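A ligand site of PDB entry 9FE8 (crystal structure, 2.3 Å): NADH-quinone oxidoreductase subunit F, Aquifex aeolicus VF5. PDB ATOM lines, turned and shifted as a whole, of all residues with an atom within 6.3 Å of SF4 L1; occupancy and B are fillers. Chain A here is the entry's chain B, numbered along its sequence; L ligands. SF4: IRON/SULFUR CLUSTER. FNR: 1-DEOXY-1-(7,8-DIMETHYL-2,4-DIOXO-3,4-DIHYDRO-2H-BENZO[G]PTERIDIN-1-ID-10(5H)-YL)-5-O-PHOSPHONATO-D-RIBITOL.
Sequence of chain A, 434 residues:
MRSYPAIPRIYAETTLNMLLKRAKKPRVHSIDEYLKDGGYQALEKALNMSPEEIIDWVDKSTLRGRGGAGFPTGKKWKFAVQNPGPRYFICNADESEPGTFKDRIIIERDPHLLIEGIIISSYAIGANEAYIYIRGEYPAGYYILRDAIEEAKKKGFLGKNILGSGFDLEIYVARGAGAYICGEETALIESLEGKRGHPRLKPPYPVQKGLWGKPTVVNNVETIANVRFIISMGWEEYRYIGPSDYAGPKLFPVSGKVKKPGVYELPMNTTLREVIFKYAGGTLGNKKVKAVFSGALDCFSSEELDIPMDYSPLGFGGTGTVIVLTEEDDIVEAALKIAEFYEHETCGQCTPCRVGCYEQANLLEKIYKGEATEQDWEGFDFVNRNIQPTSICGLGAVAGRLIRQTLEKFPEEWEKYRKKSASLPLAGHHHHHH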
ATOM      1  N   ILE A 181      16.688 -26.001  -6.356  1.00  0.00           N
ATOM      2  CA  ILE A 181      17.824 -25.181  -6.731  1.00  0.00           C
ATOM      3  C   ILE A 181      18.577 -25.829  -7.901  1.00  0.00           C
ATOM      4  O   ILE A 181      19.286 -25.131  -8.629  1.00  0.00           O
ATOM      5  CB  ILE A 181      18.746 -24.893  -5.524  1.00  0.00           C
ATOM      6  CG1 ILE A 181      19.741 -23.776  -5.812  1.00  0.00           C
ATOM      7  CG2 ILE A 181      19.466 -26.169  -5.056  1.00  0.00           C
ATOM      8  CD1 ILE A 181      19.118 -22.458  -6.243  1.00  0.00           C
ATOM      9  N   HIS A 198      24.764 -26.858  -5.447  1.00  0.00           N
ATOM     10  CA  HIS A 198      25.121 -25.560  -4.925  1.00  0.00           C
ATOM     11  C   HIS A 198      25.444 -24.658  -6.106  1.00  0.00           C
ATOM     12  O   HIS A 198      26.367 -24.942  -6.857  1.00  0.00           O
ATOM     13  CB  HIS A 198      26.337 -25.672  -4.000  1.00  0.00           C
ATOM     14  CG  HIS A 198      26.096 -26.192  -2.600  1.00  0.00           C
ATOM     15  ND1 HIS A 198      27.142 -26.475  -1.743  1.00  0.00           N
ATOM     16  CD2 HIS A 198      24.983 -26.439  -1.900  1.00  0.00           C
ATOM     17  CE1 HIS A 198      26.661 -26.882  -0.577  1.00  0.00           C
ATOM     18  NE2 HIS A 198      25.348 -26.874  -0.639  1.00  0.00           N
ATOM     19  N   PRO A 199      24.709 -23.544  -6.344  1.00  0.00           N
ATOM     20  CA  PRO A 199      25.117 -22.576  -7.356  1.00  0.00           C
ATOM     21  C   PRO A 199      26.554 -22.092  -7.192  1.00  0.00           C
ATOM     22  O   PRO A 199      27.074 -22.033  -6.078  1.00  0.00           O
ATOM     23  CB  PRO A 199      24.094 -21.440  -7.230  1.00  0.00           C
ATOM     24  CG  PRO A 199      22.880 -22.103  -6.651  1.00  0.00           C
ATOM     25  CD  PRO A 199      23.397 -23.228  -5.759  1.00  0.00           C
ATOM     26  N   ARG A 200      27.178 -21.757  -8.327  1.00  0.00           N
ATOM     27  CA  ARG A 200      28.513 -21.194  -8.377  1.00  0.00           C
ATOM     28  C   ARG A 200      28.434 -19.679  -8.541  1.00  0.00           C
ATOM     29  O   ARG A 200      27.499 -19.158  -9.129  1.00  0.00           O
ATOM     30  CB  ARG A 200      29.291 -21.666  -9.617  1.00  0.00           C
ATOM     31  CG  ARG A 200      29.410 -23.173  -9.785  1.00  0.00           C
ATOM     32  CD  ARG A 200      29.991 -23.505 -11.136  1.00  0.00           C
ATOM     33  NE  ARG A 200      30.321 -24.932 -11.237  1.00  0.00           N
ATOM     34  CZ  ARG A 200      30.783 -25.518 -12.335  1.00  0.00           C
ATOM     35  NH1 ARG A 200      30.839 -24.831 -13.474  1.00  0.00           N
ATOM     36  NH2 ARG A 200      31.161 -26.794 -12.303  1.00  0.00           N
ATOM     37  N   GLU A 345      13.759 -24.600  -0.009  1.00  0.00           N
ATOM     38  CA  GLU A 345      14.583 -24.729  -1.202  1.00  0.00           C
ATOM     39  C   GLU A 345      15.886 -23.912  -1.149  1.00  0.00           C
ATOM     40  O   GLU A 345      16.765 -24.184  -1.953  1.00  0.00           O
ATOM     41  CB  GLU A 345      13.788 -24.425  -2.480  1.00  0.00           C
ATOM     42  CG  GLU A 345      12.571 -25.341  -2.702  1.00  0.00           C
ATOM     43  CD  GLU A 345      12.848 -26.843  -2.706  1.00  0.00           C
ATOM     44  OE1 GLU A 345      14.007 -27.301  -2.881  1.00  0.00           O
ATOM     45  OE2 GLU A 345      11.861 -27.571  -2.452  1.00  0.00           O
ATOM     46  N   THR A 346      16.055 -22.964  -0.225  1.00  0.00           N
ATOM     47  CA  THR A 346      17.355 -22.315  -0.107  1.00  0.00           C
ATOM     48  C   THR A 346      18.419 -23.404   0.115  1.00  0.00           C
ATOM     49  O   THR A 346      18.197 -24.321   0.891  1.00  0.00           O
ATOM     50  CB  THR A 346      17.357 -21.263   1.007  1.00  0.00           C
ATOM     51  OG1 THR A 346      18.664 -20.712   1.026  1.00  0.00           O
ATOM     52  CG2 THR A 346      17.008 -21.849   2.361  1.00  0.00           C
ATOM     53  N   CYS A 347      19.552 -23.316  -0.573  1.00  0.00           N
ATOM     54  CA  CYS A 347      20.623 -24.303  -0.443  1.00  0.00           C
ATOM     55  C   CYS A 347      21.537 -23.992   0.736  1.00  0.00           C
ATOM     56  O   CYS A 347      22.248 -24.885   1.208  1.00  0.00           O
ATOM     57  CB  CYS A 347      21.466 -24.417  -1.701  1.00  0.00           C
ATOM     58  SG  CYS A 347      22.648 -23.074  -1.940  1.00  0.00           S
ATOM     59  N   GLY A 348      21.523 -22.738   1.172  1.00  0.00           N
ATOM     60  CA  GLY A 348      22.076 -22.339   2.452  1.00  0.00           C
ATOM     61  C   GLY A 348      23.510 -21.817   2.372  1.00  0.00           C
ATOM     62  O   GLY A 348      24.107 -21.546   3.408  1.00  0.00           O
ATOM     63  N   GLN A 349      24.050 -21.653   1.157  1.00  0.00           N
ATOM     64  CA  GLN A 349      25.422 -21.199   0.982  1.00  0.00           C
ATOM     65  C   GLN A 349      25.613 -19.766   1.461  1.00  0.00           C
ATOM     66  O   GLN A 349      26.701 -19.422   1.906  1.00  0.00           O
ATOM     67  CB  GLN A 349      25.836 -21.144  -0.484  1.00  0.00           C
ATOM     68  CG  GLN A 349      26.506 -22.383  -1.060  1.00  0.00           C
ATOM     69  CD  GLN A 349      26.798 -22.215  -2.536  1.00  0.00           C
ATOM     70  OE1 GLN A 349      25.887 -22.184  -3.374  1.00  0.00           O
ATOM     71  NE2 GLN A 349      28.074 -22.034  -2.855  1.00  0.00           N
ATOM     72  N   CYS A 350      24.617 -18.914   1.206  1.00  0.00           N
ATOM     73  CA  CYS A 350      24.660 -17.488   1.494  1.00  0.00           C
ATOM     74  C   CYS A 350      23.835 -17.230   2.759  1.00  0.00           C
ATOM     75  O   CYS A 350      22.736 -17.768   2.907  1.00  0.00           O
ATOM     76  CB  CYS A 350      24.117 -16.652   0.327  1.00  0.00           C
ATOM     77  SG  CYS A 350      24.511 -17.266  -1.331  1.00  0.00           S
ATOM     78  N   THR A 351      24.342 -16.380   3.659  1.00  0.00           N
ATOM     79  CA  THR A 351      23.788 -16.296   4.994  1.00  0.00           C
ATOM     80  C   THR A 351      22.435 -15.581   4.974  1.00  0.00           C
ATOM     81  O   THR A 351      21.488 -16.022   5.630  1.00  0.00           O
ATOM     82  CB  THR A 351      24.813 -15.670   5.962  1.00  0.00           C
ATOM     83  OG1 THR A 351      25.687 -16.722   6.340  1.00  0.00           O
ATOM     84  CG2 THR A 351      24.212 -15.099   7.232  1.00  0.00           C
ATOM     85  N   CYS A 353      20.142 -15.273   2.573  1.00  0.00           N
ATOM     86  CA  CYS A 353      19.255 -16.269   1.985  1.00  0.00           C
ATOM     87  C   CYS A 353      18.997 -17.450   2.932  1.00  0.00           C
ATOM     88  O   CYS A 353      17.839 -17.805   3.165  1.00  0.00           O
ATOM     89  CB  CYS A 353      19.787 -16.713   0.620  1.00  0.00           C
ATOM     90  SG  CYS A 353      18.752 -17.947  -0.217  1.00  0.00           S
ATOM     91  N   ARG A 354      20.041 -18.065   3.493  1.00  0.00           N
ATOM     92  CA  ARG A 354      19.853 -19.213   4.374  1.00  0.00           C
ATOM     93  C   ARG A 354      18.929 -18.842   5.531  1.00  0.00           C
ATOM     94  O   ARG A 354      17.993 -19.563   5.863  1.00  0.00           O
ATOM     95  CB  ARG A 354      21.181 -19.749   4.936  1.00  0.00           C
ATOM     96  CG  ARG A 354      21.081 -20.736   6.107  1.00  0.00           C
ATOM     97  CD  ARG A 354      22.426 -21.285   6.591  1.00  0.00           C
ATOM     98  NE  ARG A 354      23.171 -20.361   7.472  1.00  0.00           N
ATOM     99  CZ  ARG A 354      24.181 -19.604   7.083  1.00  0.00           C
ATOM    100  NH1 ARG A 354      24.615 -19.670   5.823  1.00  0.00           N
ATOM    101  NH2 ARG A 354      24.776 -18.777   7.942  1.00  0.00           N
ATOM    102  N   CYS A 357      15.073 -16.900   4.313  1.00  0.00           N
ATOM    103  CA  CYS A 357      14.047 -17.833   3.853  1.00  0.00           C
ATOM    104  C   CYS A 357      13.422 -18.576   5.049  1.00  0.00           C
ATOM    105  O   CYS A 357      12.216 -18.780   5.069  1.00  0.00           O
ATOM    106  CB  CYS A 357      14.562 -18.816   2.804  1.00  0.00           C
ATOM    107  SG  CYS A 357      14.998 -18.058   1.200  1.00  0.00           S
ATOM    108  N   ILE A 387      16.672 -10.749   2.287  1.00  0.00           N
ATOM    109  CA  ILE A 387      17.071 -12.068   1.837  1.00  0.00           C
ATOM    110  C   ILE A 387      18.121 -11.935   0.730  1.00  0.00           C
ATOM    111  O   ILE A 387      18.960 -12.820   0.576  1.00  0.00           O
ATOM    112  CB  ILE A 387      15.840 -12.859   1.368  1.00  0.00           C
ATOM    113  CG1 ILE A 387      14.710 -12.787   2.406  1.00  0.00           C
ATOM    114  CG2 ILE A 387      16.213 -14.303   1.030  1.00  0.00           C
ATOM    115  CD1 ILE A 387      13.486 -13.620   2.071  1.00  0.00           C
ATOM    116  N   THR A 390      24.221 -10.322  -0.698  1.00  0.00           N
ATOM    117  CA  THR A 390      25.362 -11.235  -0.845  1.00  0.00           C
ATOM    118  C   THR A 390      24.999 -12.489  -1.647  1.00  0.00           C
ATOM    119  O   THR A 390      25.886 -13.312  -1.878  1.00  0.00           O
ATOM    120  CB  THR A 390      26.002 -11.650   0.481  1.00  0.00           C
ATOM    121  OG1 THR A 390      25.170 -12.632   1.110  1.00  0.00           O
ATOM    122  CG2 THR A 390      26.317 -10.468   1.388  1.00  0.00           C
ATOM    123  N   SER A 391      23.730 -12.658  -2.068  1.00  0.00           N
ATOM    124  CA  SER A 391      23.318 -13.897  -2.714  1.00  0.00           C
ATOM    125  C   SER A 391      24.014 -14.062  -4.063  1.00  0.00           C
ATOM    126  O   SER A 391      24.167 -13.107  -4.813  1.00  0.00           O
ATOM    127  CB  SER A 391      21.830 -14.011  -2.859  1.00  0.00           C
ATOM    128  OG  SER A 391      21.282 -12.779  -3.276  1.00  0.00           O
ATOM    129  N   ILE A 392      24.406 -15.303  -4.356  1.00  0.00           N
ATOM    130  CA  ILE A 392      25.138 -15.609  -5.573  1.00  0.00           C
ATOM    131  C   ILE A 392      24.242 -16.247  -6.623  1.00  0.00           C
ATOM    132  O   ILE A 392      24.774 -16.664  -7.645  1.00  0.00           O
ATOM    133  CB  ILE A 392      26.374 -16.483  -5.254  1.00  0.00           C
ATOM    134  CG1 ILE A 392      26.008 -17.912  -4.781  1.00  0.00           C
ATOM    135  CG2 ILE A 392      27.283 -15.774  -4.263  1.00  0.00           C
ATOM    136  CD1 ILE A 392      27.195 -18.728  -4.310  1.00  0.00           C
ATOM    137  N   CYS A 393      22.927 -16.350  -6.385  1.00  0.00           N
ATOM    138  CA  CYS A 393      21.984 -16.892  -7.372  1.00  0.00           C
ATOM    139  C   CYS A 393      20.643 -16.199  -7.184  1.00  0.00           C
ATOM    140  O   CYS A 393      20.480 -15.442  -6.226  1.00  0.00           O
ATOM    141  CB  CYS A 393      21.860 -18.419  -7.319  1.00  0.00           C
ATOM    142  SG  CYS A 393      20.451 -19.080  -6.359  1.00  0.00           S
ATOM    143  N   GLY A 394      19.694 -16.444  -8.088  1.00  0.00           N
ATOM    144  CA  GLY A 394      18.471 -15.652  -8.189  1.00  0.00           C
ATOM    145  C   GLY A 394      17.405 -16.029  -7.147  1.00  0.00           C
ATOM    146  O   GLY A 394      16.506 -15.241  -6.897  1.00  0.00           O
ATOM    147  N   LEU A 395      17.531 -17.217  -6.517  1.00  0.00           N
ATOM    148  CA  LEU A 395      16.601 -17.627  -5.480  1.00  0.00           C
ATOM    149  C   LEU A 395      16.575 -16.586  -4.371  1.00  0.00           C
ATOM    150  O   LEU A 395      15.516 -16.175  -3.907  1.00  0.00           O
ATOM    151  CB  LEU A 395      16.947 -19.005  -4.927  1.00  0.00           C
ATOM    152  CG  LEU A 395      15.867 -19.640  -4.058  1.00  0.00           C
ATOM    153  CD1 LEU A 395      15.930 -21.170  -4.112  1.00  0.00           C
ATOM    154  CD2 LEU A 395      15.969 -19.146  -2.628  1.00  0.00           C
ATOM    155  N   GLY A 396      17.763 -16.163  -3.929  1.00  0.00           N
ATOM    156  CA  GLY A 396      17.851 -15.222  -2.834  1.00  0.00           C
ATOM    157  C   GLY A 396      17.352 -13.860  -3.269  1.00  0.00           C
ATOM    158  O   GLY A 396      16.773 -13.133  -2.474  1.00  0.00           O
ATOM    159  N   ALA A 397      17.542 -13.560  -4.554  1.00  0.00           N
ATOM    160  CA  ALA A 397      17.048 -12.321  -5.150  1.00  0.00           C
ATOM    161  C   ALA A 397      15.517 -12.217  -5.123  1.00  0.00           C
ATOM    162  O   ALA A 397      14.989 -11.120  -5.036  1.00  0.00           O
ATOM    163  CB  ALA A 397      17.593 -12.201  -6.570  1.00  0.00           C
HETATM  164 FE1  SF4 L   1      21.178 -19.130  -4.190  1.00  0.00          FE
HETATM  165 FE2  SF4 L   1      22.798 -18.451  -2.185  1.00  0.00          FE
HETATM  166 FE3  SF4 L   1      21.836 -20.999  -2.312  1.00  0.00          FE
HETATM  167 FE4  SF4 L   1      20.197 -18.880  -1.663  1.00  0.00          FE
HETATM  168  S1  SF4 L   1      21.920 -19.695  -0.467  1.00  0.00           S
HETATM  169  S2  SF4 L   1      19.733 -20.572  -3.127  1.00  0.00           S
HETATM  170  S3  SF4 L   1      21.076 -17.244  -2.975  1.00  0.00           S
HETATM  171  S4  SF4 L   1      23.252 -19.950  -3.791  1.00  0.00           S
HETATM  172  C9A FNR L   2      16.149 -21.594 -12.609  1.00  0.00           C
HETATM  173  N10 FNR L   2      16.085 -21.853 -13.994  1.00  0.00           N
HETATM  174  CAA FNR L   2      15.392 -22.948 -14.449  1.00  0.00           C
HETATM  175  N1  FNR L   2      15.388 -23.192 -15.789  1.00  0.00           N
HETATM  176  C2  FNR L   2      14.790 -24.279 -16.338  1.00  0.00           C
HETATM  177  O2  FNR L   2      14.875 -24.532 -17.532  1.00  0.00           O
HETATM  178  N3  FNR L   2      14.131 -25.100 -15.458  1.00  0.00           N
HETATM  179  C4  FNR L   2      14.044 -24.957 -14.087  1.00  0.00           C
HETATM  180  O4  FNR L   2      13.395 -25.758 -13.439  1.00  0.00           O
HETATM  181  C4A FNR L   2      14.740 -23.808 -13.581  1.00  0.00           C
HETATM  182  N5  FNR L   2      14.784 -23.579 -12.246  1.00  0.00           N
HETATM  183  C5A FNR L   2      15.503 -22.484 -11.734  1.00  0.00           C
HETATM  184  C6  FNR L   2      15.564 -22.270 -10.354  1.00  0.00           C
HETATM  185  C7  FNR L   2      16.269 -21.185  -9.841  1.00  0.00           C
HETATM  186  C7M FNR L   2      16.287 -20.952  -8.347  1.00  0.00           C
HETATM  187  C8  FNR L   2      16.910 -20.298 -10.725  1.00  0.00           C
HETATM  188  C8M FNR L   2      17.621 -19.061 -10.214  1.00  0.00           C
HETATM  189  C9  FNR L   2      16.844 -20.515 -12.089  1.00  0.00           C
HETATM  190  C1' FNR L   2      16.787 -20.982 -14.955  1.00  0.00           C
HETATM  191  C2' FNR L   2      18.114 -21.593 -15.387  1.00  0.00           C
HETATM  192  O2' FNR L   2      19.126 -21.218 -14.448  1.00  0.00           O
HETATM  193  C3' FNR L   2      18.475 -21.093 -16.787  1.00  0.00           C
HETATM  194  O3' FNR L   2      18.163 -19.709 -16.912  1.00  0.00           O
HETATM  195  C4' FNR L   2      17.733 -21.828 -17.914  1.00  0.00           C
HETATM  196  O4' FNR L   2      17.637 -23.235 -17.678  1.00  0.00           O
HETATM  197  C5' FNR L   2      18.381 -21.524 -19.245  1.00  0.00           C
HETATM  198  O5' FNR L   2      17.569 -22.050 -20.302  1.00  0.00           O
HETATM  199  P   FNR L   2      16.746 -21.011 -21.240  1.00  0.00           P
HETATM  200  O1P FNR L   2      16.246 -21.939 -22.346  1.00  0.00           O
HETATM  201  O2P FNR L   2      17.743 -19.984 -21.738  1.00  0.00           O
HETATM  202  O3P FNR L   2      15.631 -20.395 -20.433  1.00  0.00           O
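The side-chain sulfur (SG) of Cys 353 binds an iron atom (FE4) of SF4 L1 (2.2 Å).
FE2 of SF4 L1 is bound by SG of Cys 350, 2.3 Å away.
OG1 of Thr 346 sits close to S1 of SF4 L1, 3.7 Å away.
The backbone NH (N) of Gly 396 sits close to a sulfur (S3) of SF4 L1.
An iron atom (FE3) of SF4 L1 is bound by the side-chain sulfur of Cys 347.
The side-chain amide oxygen (OE1) of Gln 349 lies close to a sulfur (S4) of SF4 L1 (3.5 Å).
A sulfur (S2) of SF4 L1 lies close to the backbone NH (N) of Cys 347, 3.8 Å away.
A sulfur (S1) of SF4 L1 sits close to the backbone NH (N) of Gln 349.
The backbone NH (N) of Gly 348 lies close to a sulfur (S1) of SF4 L1, 3.5 Å away.
SG of Cys 393 binds FE1 of SF4 L1.
N of Cys 350 sits close to S1 of SF4 L1.
Ile 181 touches SF4 L1 (CD1 to S2, 3.7 Å).
Pro 199 touches SF4 L1 (CG to S4, 3.6 Å).
CB of Ser 391 touches S3 of SF4 L1, 3.3 Å away.
CG1 of Ile 392 touches S4 of SF4 L1, 3.6 Å away.
Leu 395 touches SF4 L1 (CB to S2, 3.7 Å).
Hydrophobic or aromatic side chains within 4 Å of SF4 L1: Ile 181, Pro 199, Ile 392 and Leu 395.
The guanidinium group of Arg 354 is in hydrogen-bond range of the backbone carbonyl oxygen of Gly 348, at 3.1 Å.
SG of Cys 357 lies close to O of Cys 353 (3.5 Å).
The backbone NH (N) of Cys 353 sits at hydrogen-bond distance from the backbone carbonyl oxygen (O) of Ile 387 (3.4 Å).
The backbone NH (N) of Ile 392 sits close to the side-chain sulfur (SG) of Cys 350, 3.6 Å away.
SG of Cys 393 lies close to N of Leu 395.
SG of Cys 353 lies close to OG1 of Thr 346, at 3.0 Å.
The side-chain sulfur (SG) of Cys 347 sits close to the side-chain amide oxygen (OE1) of Gln 349.
The side-chain amide oxygen of Gln 349 sits close to the backbone carbonyl oxygen of Pro 199, at 3.0 Å.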
